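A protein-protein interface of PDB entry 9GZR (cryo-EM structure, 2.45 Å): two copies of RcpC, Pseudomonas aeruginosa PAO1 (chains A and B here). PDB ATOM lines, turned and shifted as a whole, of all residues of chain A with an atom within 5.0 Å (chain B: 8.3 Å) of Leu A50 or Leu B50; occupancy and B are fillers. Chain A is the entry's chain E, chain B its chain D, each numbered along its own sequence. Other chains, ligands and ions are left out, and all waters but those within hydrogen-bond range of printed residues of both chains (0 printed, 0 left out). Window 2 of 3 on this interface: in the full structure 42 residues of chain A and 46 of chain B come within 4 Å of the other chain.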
ATOM      1  N   LYS A  25     -22.839  22.586 -12.313  1.00  0.00           N
ATOM      2  CA  LYS A  25     -21.591  21.841 -12.443  1.00  0.00           C
ATOM      3  C   LYS A  25     -20.342  22.570 -11.911  1.00  0.00           C
ATOM      4  O   LYS A  25     -19.544  21.953 -11.208  1.00  0.00           O
ATOM      5  CB  LYS A  25     -21.368  21.436 -13.903  1.00  0.00           C
ATOM      6  CG  LYS A  25     -21.937  20.075 -14.257  1.00  0.00           C
ATOM      7  CD  LYS A  25     -21.101  19.389 -15.320  1.00  0.00           C
ATOM      8  CE  LYS A  25     -21.761  18.110 -15.796  1.00  0.00           C
ATOM      9  NZ  LYS A  25     -23.109  18.362 -16.371  1.00  0.00           N
ATOM     10  N   VAL A  27     -18.037  24.631  -9.487  1.00  0.00           N
ATOM     11  CA  VAL A  27     -18.034  24.821  -8.043  1.00  0.00           C
ATOM     12  C   VAL A  27     -16.664  25.338  -7.627  1.00  0.00           C
ATOM     13  O   VAL A  27     -15.628  24.879  -8.118  1.00  0.00           O
ATOM     14  CB  VAL A  27     -18.391  23.510  -7.303  1.00  0.00           C
ATOM     15  CG1 VAL A  27     -17.753  23.463  -5.924  1.00  0.00           C
ATOM     16  CG2 VAL A  27     -19.896  23.352  -7.200  1.00  0.00           C
ATOM     17  N   GLU A  48     -13.732  23.657  -9.946  1.00  0.00           N
ATOM     18  CA  GLU A  48     -13.848  22.233 -10.210  1.00  0.00           C
ATOM     19  C   GLU A  48     -15.238  21.919 -10.749  1.00  0.00           C
ATOM     20  O   GLU A  48     -16.225  22.558 -10.381  1.00  0.00           O
ATOM     21  CB  GLU A  48     -13.583  21.412  -8.947  1.00  0.00           C
ATOM     22  CG  GLU A  48     -12.291  21.768  -8.233  1.00  0.00           C
ATOM     23  CD  GLU A  48     -11.258  20.665  -8.320  1.00  0.00           C
ATOM     24  OE1 GLU A  48     -11.343  19.844  -9.256  1.00  0.00           O
ATOM     25  OE2 GLU A  48     -10.362  20.616  -7.452  1.00  0.00           O
ATOM     26  N   LEU A  49     -15.307  20.926 -11.627  1.00  0.00           N
ATOM     27  CA  LEU A  49     -16.559  20.529 -12.257  1.00  0.00           C
ATOM     28  C   LEU A  49     -17.081  19.281 -11.554  1.00  0.00           C
ATOM     29  O   LEU A  49     -16.500  18.200 -11.681  1.00  0.00           O
ATOM     30  CB  LEU A  49     -16.360  20.287 -13.751  1.00  0.00           C
ATOM     31  CG  LEU A  49     -16.357  21.551 -14.612  1.00  0.00           C
ATOM     32  CD1 LEU A  49     -15.507  21.352 -15.855  1.00  0.00           C
ATOM     33  CD2 LEU A  49     -17.774  21.954 -14.985  1.00  0.00           C
ATOM     34  N   LEU A  50     -18.176  19.436 -10.816  1.00  0.00           N
ATOM     35  CA  LEU A  50     -18.783  18.360 -10.051  1.00  0.00           C
ATOM     36  C   LEU A  50     -20.156  18.029 -10.617  1.00  0.00           C
ATOM     37  O   LEU A  50     -20.833  18.886 -11.190  1.00  0.00           O
ATOM     38  CB  LEU A  50     -18.907  18.745  -8.576  1.00  0.00           C
ATOM     39  CG  LEU A  50     -17.608  19.125  -7.871  1.00  0.00           C
ATOM     40  CD1 LEU A  50     -17.856  19.371  -6.395  1.00  0.00           C
ATOM     41  CD2 LEU A  50     -16.560  18.044  -8.066  1.00  0.00           C
ATOM     42  N   ARG A  51     -20.560  16.767 -10.458  1.00  0.00           N
ATOM     43  CA  ARG A  51     -21.847  16.331 -10.991  1.00  0.00           C
ATOM     44  C   ARG A  51     -23.008  17.013 -10.281  1.00  0.00           C
ATOM     45  O   ARG A  51     -24.006  17.371 -10.918  1.00  0.00           O
ATOM     46  CB  ARG A  51     -21.969  14.811 -10.894  1.00  0.00           C
ATOM     47  CG  ARG A  51     -21.763  14.099 -12.220  1.00  0.00           C
ATOM     48  CD  ARG A  51     -21.839  12.590 -12.067  1.00  0.00           C
ATOM     49  NE  ARG A  51     -20.835  12.085 -11.139  1.00  0.00           N
ATOM     50  CZ  ARG A  51     -19.938  11.156 -11.442  1.00  0.00           C
ATOM     51  NH1 ARG A  51     -19.890  10.608 -12.645  1.00  0.00           N
ATOM     52  NH2 ARG A  51     -19.064  10.771 -10.516  1.00  0.00           N
ATOM     53  N   THR A  52     -22.906  17.197  -8.970  1.00  0.00           N
ATOM     54  CA  THR A  52     -23.923  17.892  -8.195  1.00  0.00           C
ATOM     55  C   THR A  52     -23.292  19.035  -7.411  1.00  0.00           C
ATOM     56  O   THR A  52     -22.222  18.878  -6.815  1.00  0.00           O
ATOM     57  CB  THR A  52     -24.643  16.931  -7.245  1.00  0.00           C
ATOM     58  OG1 THR A  52     -25.405  17.680  -6.292  1.00  0.00           O
ATOM     59  CG2 THR A  52     -23.647  16.036  -6.525  1.00  0.00           C
ATOM     60  N   ILE A  78     -15.026  22.886  -0.343  1.00  0.00           N
ATOM     61  CA  ILE A  78     -15.999  23.674  -1.080  1.00  0.00           C
ATOM     62  C   ILE A  78     -16.360  24.907  -0.260  1.00  0.00           C
ATOM     63  O   ILE A  78     -16.652  24.825   0.939  1.00  0.00           O
ATOM     64  CB  ILE A  78     -17.251  22.845  -1.411  1.00  0.00           C
ATOM     65  CG1 ILE A  78     -16.864  21.595  -2.200  1.00  0.00           C
ATOM     66  CG2 ILE A  78     -18.252  23.678  -2.191  1.00  0.00           C
ATOM     67  CD1 ILE A  78     -18.029  20.912  -2.874  1.00  0.00           C
ATOM     68  N   GLU B  23      -9.118  14.814 -12.122  1.00  0.00           N
ATOM     69  CA  GLU B  23      -7.933  15.581 -12.474  1.00  0.00           C
ATOM     70  C   GLU B  23      -6.700  15.035 -11.761  1.00  0.00           C
ATOM     71  O   GLU B  23      -5.590  15.113 -12.286  1.00  0.00           O
ATOM     72  CB  GLU B  23      -8.137  17.059 -12.139  1.00  0.00           C
ATOM     73  CG  GLU B  23      -9.420  17.640 -12.714  1.00  0.00           C
ATOM     74  CD  GLU B  23      -9.408  19.154 -12.770  1.00  0.00           C
ATOM     75  OE1 GLU B  23      -8.439  19.761 -12.272  1.00  0.00           O
ATOM     76  OE2 GLU B  23     -10.370  19.736 -13.312  1.00  0.00           O
ATOM     77  N   ARG B  24      -6.901  14.477 -10.567  1.00  0.00           N
ATOM     78  CA  ARG B  24      -5.805  13.866  -9.825  1.00  0.00           C
ATOM     79  C   ARG B  24      -6.318  12.896  -8.765  1.00  0.00           C
ATOM     80  O   ARG B  24      -6.582  11.727  -9.063  1.00  0.00           O
ATOM     81  CB  ARG B  24      -4.927  14.943  -9.184  1.00  0.00           C
ATOM     82  CG  ARG B  24      -3.590  14.439  -8.657  1.00  0.00           C
ATOM     83  CD  ARG B  24      -2.864  13.563  -9.667  1.00  0.00           C
ATOM     84  NE  ARG B  24      -2.341  14.326 -10.793  1.00  0.00           N
ATOM     85  CZ  ARG B  24      -2.651  14.098 -12.061  1.00  0.00           C
ATOM     86  NH1 ARG B  24      -3.483  13.130 -12.406  1.00  0.00           N
ATOM     87  NH2 ARG B  24      -2.110  14.860 -13.008  1.00  0.00           N
ATOM     88  N   LYS B  25      -6.466  13.367  -7.527  1.00  0.00           N
ATOM     89  CA  LYS B  25      -6.811  12.485  -6.425  1.00  0.00           C
ATOM     90  C   LYS B  25      -8.315  12.220  -6.375  1.00  0.00           C
ATOM     91  O   LYS B  25      -9.122  13.081  -6.730  1.00  0.00           O
ATOM     92  CB  LYS B  25      -6.345  13.086  -5.103  1.00  0.00           C
ATOM     93  CG  LYS B  25      -4.842  13.242  -4.993  1.00  0.00           C
ATOM     94  CD  LYS B  25      -4.442  13.809  -3.644  1.00  0.00           C
ATOM     95  CE  LYS B  25      -4.448  15.329  -3.660  1.00  0.00           C
ATOM     96  NZ  LYS B  25      -4.047  15.902  -2.345  1.00  0.00           N
ATOM     97  N   PRO B  26      -8.717  11.028  -5.916  1.00  0.00           N
ATOM     98  CA  PRO B  26     -10.149  10.727  -5.792  1.00  0.00           C
ATOM     99  C   PRO B  26     -10.700  11.040  -4.408  1.00  0.00           C
ATOM    100  O   PRO B  26     -10.031  10.810  -3.397  1.00  0.00           O
ATOM    101  CB  PRO B  26     -10.215   9.225  -6.095  1.00  0.00           C
ATOM    102  CG  PRO B  26      -8.802   8.703  -5.876  1.00  0.00           C
ATOM    103  CD  PRO B  26      -7.889   9.862  -5.576  1.00  0.00           C
ATOM    104  N   VAL B  27     -11.923  11.562  -4.354  1.00  0.00           N
ATOM    105  CA  VAL B  27     -12.578  11.939  -3.108  1.00  0.00           C
ATOM    106  C   VAL B  27     -14.018  11.443  -3.155  1.00  0.00           C
ATOM    107  O   VAL B  27     -14.683  11.542  -4.194  1.00  0.00           O
ATOM    108  CB  VAL B  27     -12.526  13.463  -2.875  1.00  0.00           C
ATOM    109  CG1 VAL B  27     -13.437  13.871  -1.729  1.00  0.00           C
ATOM    110  CG2 VAL B  27     -11.101  13.906  -2.597  1.00  0.00           C
ATOM    111  N   LEU B  28     -14.488  10.902  -2.034  1.00  0.00           N
ATOM    112  CA  LEU B  28     -15.839  10.372  -1.930  1.00  0.00           C
ATOM    113  C   LEU B  28     -16.811  11.477  -1.533  1.00  0.00           C
ATOM    114  O   LEU B  28     -16.572  12.216  -0.575  1.00  0.00           O
ATOM    115  CB  LEU B  28     -15.875   9.248  -0.895  1.00  0.00           C
ATOM    116  CG  LEU B  28     -15.974   7.794  -1.356  1.00  0.00           C
ATOM    117  CD1 LEU B  28     -16.383   6.916  -0.194  1.00  0.00           C
ATOM    118  CD2 LEU B  28     -16.943   7.637  -2.505  1.00  0.00           C
ATOM    119  N   VAL B  29     -17.913  11.589  -2.277  1.00  0.00           N
ATOM    120  CA  VAL B  29     -18.935  12.601  -2.043  1.00  0.00           C
ATOM    121  C   VAL B  29     -20.301  11.927  -2.038  1.00  0.00           C
ATOM    122  O   VAL B  29     -20.468  10.803  -2.513  1.00  0.00           O
ATOM    123  CB  VAL B  29     -18.906  13.729  -3.097  1.00  0.00           C
ATOM    124  CG1 VAL B  29     -17.516  14.334  -3.205  1.00  0.00           C
ATOM    125  CG2 VAL B  29     -19.373  13.208  -4.441  1.00  0.00           C
ATOM    126  N   VAL B  47     -17.785   9.054  -6.547  1.00  0.00           N
ATOM    127  CA  VAL B  47     -16.366   9.388  -6.519  1.00  0.00           C
ATOM    128  C   VAL B  47     -16.116  10.532  -7.493  1.00  0.00           C
ATOM    129  O   VAL B  47     -16.665  10.547  -8.600  1.00  0.00           O
ATOM    130  CB  VAL B  47     -15.491   8.163  -6.842  1.00  0.00           C
ATOM    131  CG1 VAL B  47     -15.696   7.697  -8.275  1.00  0.00           C
ATOM    132  CG2 VAL B  47     -14.026   8.474  -6.582  1.00  0.00           C
ATOM    133  N   GLU B  48     -15.320  11.510  -7.064  1.00  0.00           N
ATOM    134  CA  GLU B  48     -14.969  12.649  -7.897  1.00  0.00           C
ATOM    135  C   GLU B  48     -13.466  12.877  -7.852  1.00  0.00           C
ATOM    136  O   GLU B  48     -12.831  12.726  -6.806  1.00  0.00           O
ATOM    137  CB  GLU B  48     -15.701  13.918  -7.448  1.00  0.00           C
ATOM    138  CG  GLU B  48     -17.212  13.795  -7.457  1.00  0.00           C
ATOM    139  CD  GLU B  48     -17.848  14.536  -8.614  1.00  0.00           C
ATOM    140  OE1 GLU B  48     -17.371  14.376  -9.755  1.00  0.00           O
ATOM    141  OE2 GLU B  48     -18.825  15.278  -8.382  1.00  0.00           O
ATOM    142  N   LEU B  49     -12.897  13.258  -8.990  1.00  0.00           N
ATOM    143  CA  LEU B  49     -11.460  13.456  -9.111  1.00  0.00           C
ATOM    144  C   LEU B  49     -11.148  14.946  -9.051  1.00  0.00           C
ATOM    145  O   LEU B  49     -11.630  15.720  -9.884  1.00  0.00           O
ATOM    146  CB  LEU B  49     -10.939  12.837 -10.407  1.00  0.00           C
ATOM    147  CG  LEU B  49     -11.229  11.348 -10.580  1.00  0.00           C
ATOM    148  CD1 LEU B  49     -12.305  11.130 -11.630  1.00  0.00           C
ATOM    149  CD2 LEU B  49      -9.961  10.594 -10.939  1.00  0.00           C
ATOM    150  N   LEU B  50     -10.342  15.339  -8.069  1.00  0.00           N
ATOM    151  CA  LEU B  50     -10.037  16.737  -7.810  1.00  0.00           C
ATOM    152  C   LEU B  50      -8.528  16.922  -7.780  1.00  0.00           C
ATOM    153  O   LEU B  50      -7.764  15.956  -7.714  1.00  0.00           O
ATOM    154  CB  LEU B  50     -10.638  17.216  -6.482  1.00  0.00           C
ATOM    155  CG  LEU B  50     -11.933  16.577  -5.979  1.00  0.00           C
ATOM    156  CD1 LEU B  50     -12.228  17.045  -4.568  1.00  0.00           C
ATOM    157  CD2 LEU B  50     -13.095  16.897  -6.899  1.00  0.00           C
ATOM    158  N   ARG B  51      -8.102  18.185  -7.828  1.00  0.00           N
ATOM    159  CA  ARG B  51      -6.675  18.480  -7.747  1.00  0.00           C
ATOM    160  C   ARG B  51      -6.138  18.247  -6.343  1.00  0.00           C
ATOM    161  O   ARG B  51      -5.015  17.755  -6.176  1.00  0.00           O
ATOM    162  CB  ARG B  51      -6.402  19.916  -8.191  1.00  0.00           C
ATOM    163  CG  ARG B  51      -6.665  20.171  -9.662  1.00  0.00           C
ATOM    164  CD  ARG B  51      -6.969  21.635  -9.928  1.00  0.00           C
ATOM    165  NE  ARG B  51      -5.833  22.492  -9.613  1.00  0.00           N
ATOM    166  CZ  ARG B  51      -5.230  23.288 -10.485  1.00  0.00           C
ATOM    167  NH1 ARG B  51      -5.629  23.361 -11.745  1.00  0.00           N
ATOM    168  NH2 ARG B  51      -4.200  24.028 -10.085  1.00  0.00           N
ATOM    169  N   THR B  52      -6.915  18.594  -5.323  1.00  0.00           N
ATOM    170  CA  THR B  52      -6.480  18.493  -3.938  1.00  0.00           C
ATOM    171  C   THR B  52      -7.546  17.804  -3.097  1.00  0.00           C
ATOM    172  O   THR B  52      -8.744  17.950  -3.352  1.00  0.00           O
ATOM    173  CB  THR B  52      -6.156  19.874  -3.364  1.00  0.00           C
ATOM    174  OG1 THR B  52      -5.754  19.748  -1.995  1.00  0.00           O
ATOM    175  CG2 THR B  52      -7.349  20.800  -3.479  1.00  0.00           C
ATOM    176  N   ALA B  53      -7.094  17.042  -2.101  1.00  0.00           N
ATOM    177  CA  ALA B  53      -7.980  16.254  -1.261  1.00  0.00           C
ATOM    178  C   ALA B  53      -7.992  16.822   0.145  1.00  0.00           C
ATOM    179  O   ALA B  53      -6.925  16.914   0.772  1.00  0.00           O
ATOM    180  CB  ALA B  53      -7.539  14.797  -1.235  1.00  0.00           C
ATOM    181  N   PRO B  54      -9.145  17.217   0.677  1.00  0.00           N
ATOM    182  CA  PRO B  54      -9.183  17.781   2.027  1.00  0.00           C
ATOM    183  C   PRO B  54      -8.806  16.758   3.084  1.00  0.00           C
ATOM    184  O   PRO B  54      -8.960  15.550   2.900  1.00  0.00           O
ATOM    185  CB  PRO B  54     -10.643  18.219   2.181  1.00  0.00           C
ATOM    186  CG  PRO B  54     -11.121  18.396   0.777  1.00  0.00           C
ATOM    187  CD  PRO B  54     -10.465  17.281   0.032  1.00  0.00           C
ATOM    188  N   SER B  57     -10.997  13.297   4.216  1.00  0.00           N
ATOM    189  CA  SER B  57     -11.729  12.640   3.147  1.00  0.00           C
ATOM    190  C   SER B  57     -11.296  11.180   3.016  1.00  0.00           C
ATOM    191  O   SER B  57     -10.308  10.736   3.607  1.00  0.00           O
ATOM    192  CB  SER B  57     -11.520  13.380   1.827  1.00  0.00           C
ATOM    193  OG  SER B  57     -10.203  13.894   1.735  1.00  0.00           O
ATOM    194  N   GLY B  76     -24.160  16.381  -2.618  1.00  0.00           N
ATOM    195  CA  GLY B  76     -22.912  16.884  -3.144  1.00  0.00           C
ATOM    196  C   GLY B  76     -21.851  17.196  -2.116  1.00  0.00           C
ATOM    197  O   GLY B  76     -20.745  17.593  -2.497  1.00  0.00           O
ATOM    198  N   SER B  77     -22.141  17.033  -0.831  1.00  0.00           N
ATOM    199  CA  SER B  77     -21.173  17.371   0.201  1.00  0.00           C
ATOM    200  C   SER B  77     -20.028  16.368   0.206  1.00  0.00           C
ATOM    201  O   SER B  77     -20.218  15.188  -0.100  1.00  0.00           O
ATOM    202  CB  SER B  77     -21.849  17.410   1.568  1.00  0.00           C
ATOM    203  OG  SER B  77     -22.935  18.316   1.573  1.00  0.00           O
ATOM    204  N   ILE B  78     -18.833  16.844   0.548  1.00  0.00           N
ATOM    205  CA  ILE B  78     -17.682  15.961   0.683  1.00  0.00           C
ATOM    206  C   ILE B  78     -17.782  15.236   2.016  1.00  0.00           C
ATOM    207  O   ILE B  78     -17.906  15.864   3.073  1.00  0.00           O
ATOM    208  CB  ILE B  78     -16.371  16.749   0.571  1.00  0.00           C
ATOM    209  CG1 ILE B  78     -16.086  17.105  -0.887  1.00  0.00           C
ATOM    210  CG2 ILE B  78     -15.218  15.959   1.159  1.00  0.00           C
ATOM    211  CD1 ILE B  78     -14.770  17.814  -1.092  1.00  0.00           C
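The guanidinium group (NH2) of Arg A51 lies within hydrogen-bond range of the backbone carbonyl oxygen (O) of Val B47, 3.1 Å away. The backbone NH (N) of Arg B51 lies within hydrogen-bond range of the side-chain carboxylate (OE2) of Glu A48, 3.3 Å away. The backbone NH (N) of Arg A51 sits at hydrogen-bond distance from the side-chain carboxylate (OE2) of Glu B48.
The backbone carbonyl oxygen (O) of Lys B25 sits at hydrogen-bond distance from the backbone NH (N) of Leu B50 (2.9 Å). The backbone NH (N) of Arg B24 is in hydrogen-bond range of the backbone carbonyl oxygen (O) of Leu B50 (3.3 Å). N of Val B27 is in hydrogen-bond range of O of Glu B48. O of Glu A48 is in hydrogen-bond range of N of Val A27 (2.9 Å). The backbone carbonyl oxygen of Lys A25 lies within hydrogen-bond range of the backbone NH of Leu A50 (2.9 Å).
CB of Leu B50 touches OE2 of Glu A48, at 3.5 Å. Leu A50 touches Glu B48. Leu A50 touches Leu B50 (CD2 to CD2, 3.8 Å). Gly B76 touches Thr A52 (CA to CG2, 3.6 Å).
Of the printed residues of chain B, Glu A48 touches Leu B50 (3.5 Å) and Arg B51 (3.3 Å). Of chain B, only Glu B48 and Leu B50 come within 4 Å of Leu A50. Printed residues of chain A within 4 Å of Val B47: Arg A51 (3.1 Å). Printed residues of chain A within 4 Å of Leu B50: Glu A48 and Leu A50. Thr B52 touches none of the printed residues of chain A. Ala B53 touches none of the printed residues of chain A. The nearest printed residue of chain A that does not touch Leu B50 is Leu A49 (6.0 Å).
Of the 19 printed residues of chain B, 5 touch a printed residue of chain A. Hydrophobic or aromatic side chains of chain B that line the printed part of chain A: Leu B50. Of the 8 printed residues of chain A, 4 touch a printed residue of chain B. Among the printed residues, 7 pairs touch across the chains. Among the printed residues, no Asp or Glu carboxylate lies within 4 Å of a Lys or Arg side-chain nitrogen of the other chain.
Glu A48 touches Leu B50, and with the chains exchanged Leu A50 touches Glu B48. Glu A48 touches Arg B51, and with the chains exchanged Arg A51 touches Glu B48. Leu A50 touches its own counterpart, Leu B50. Positions printed for both chains: 25, 27, 48, 49, 50, 51, 52 and 78.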
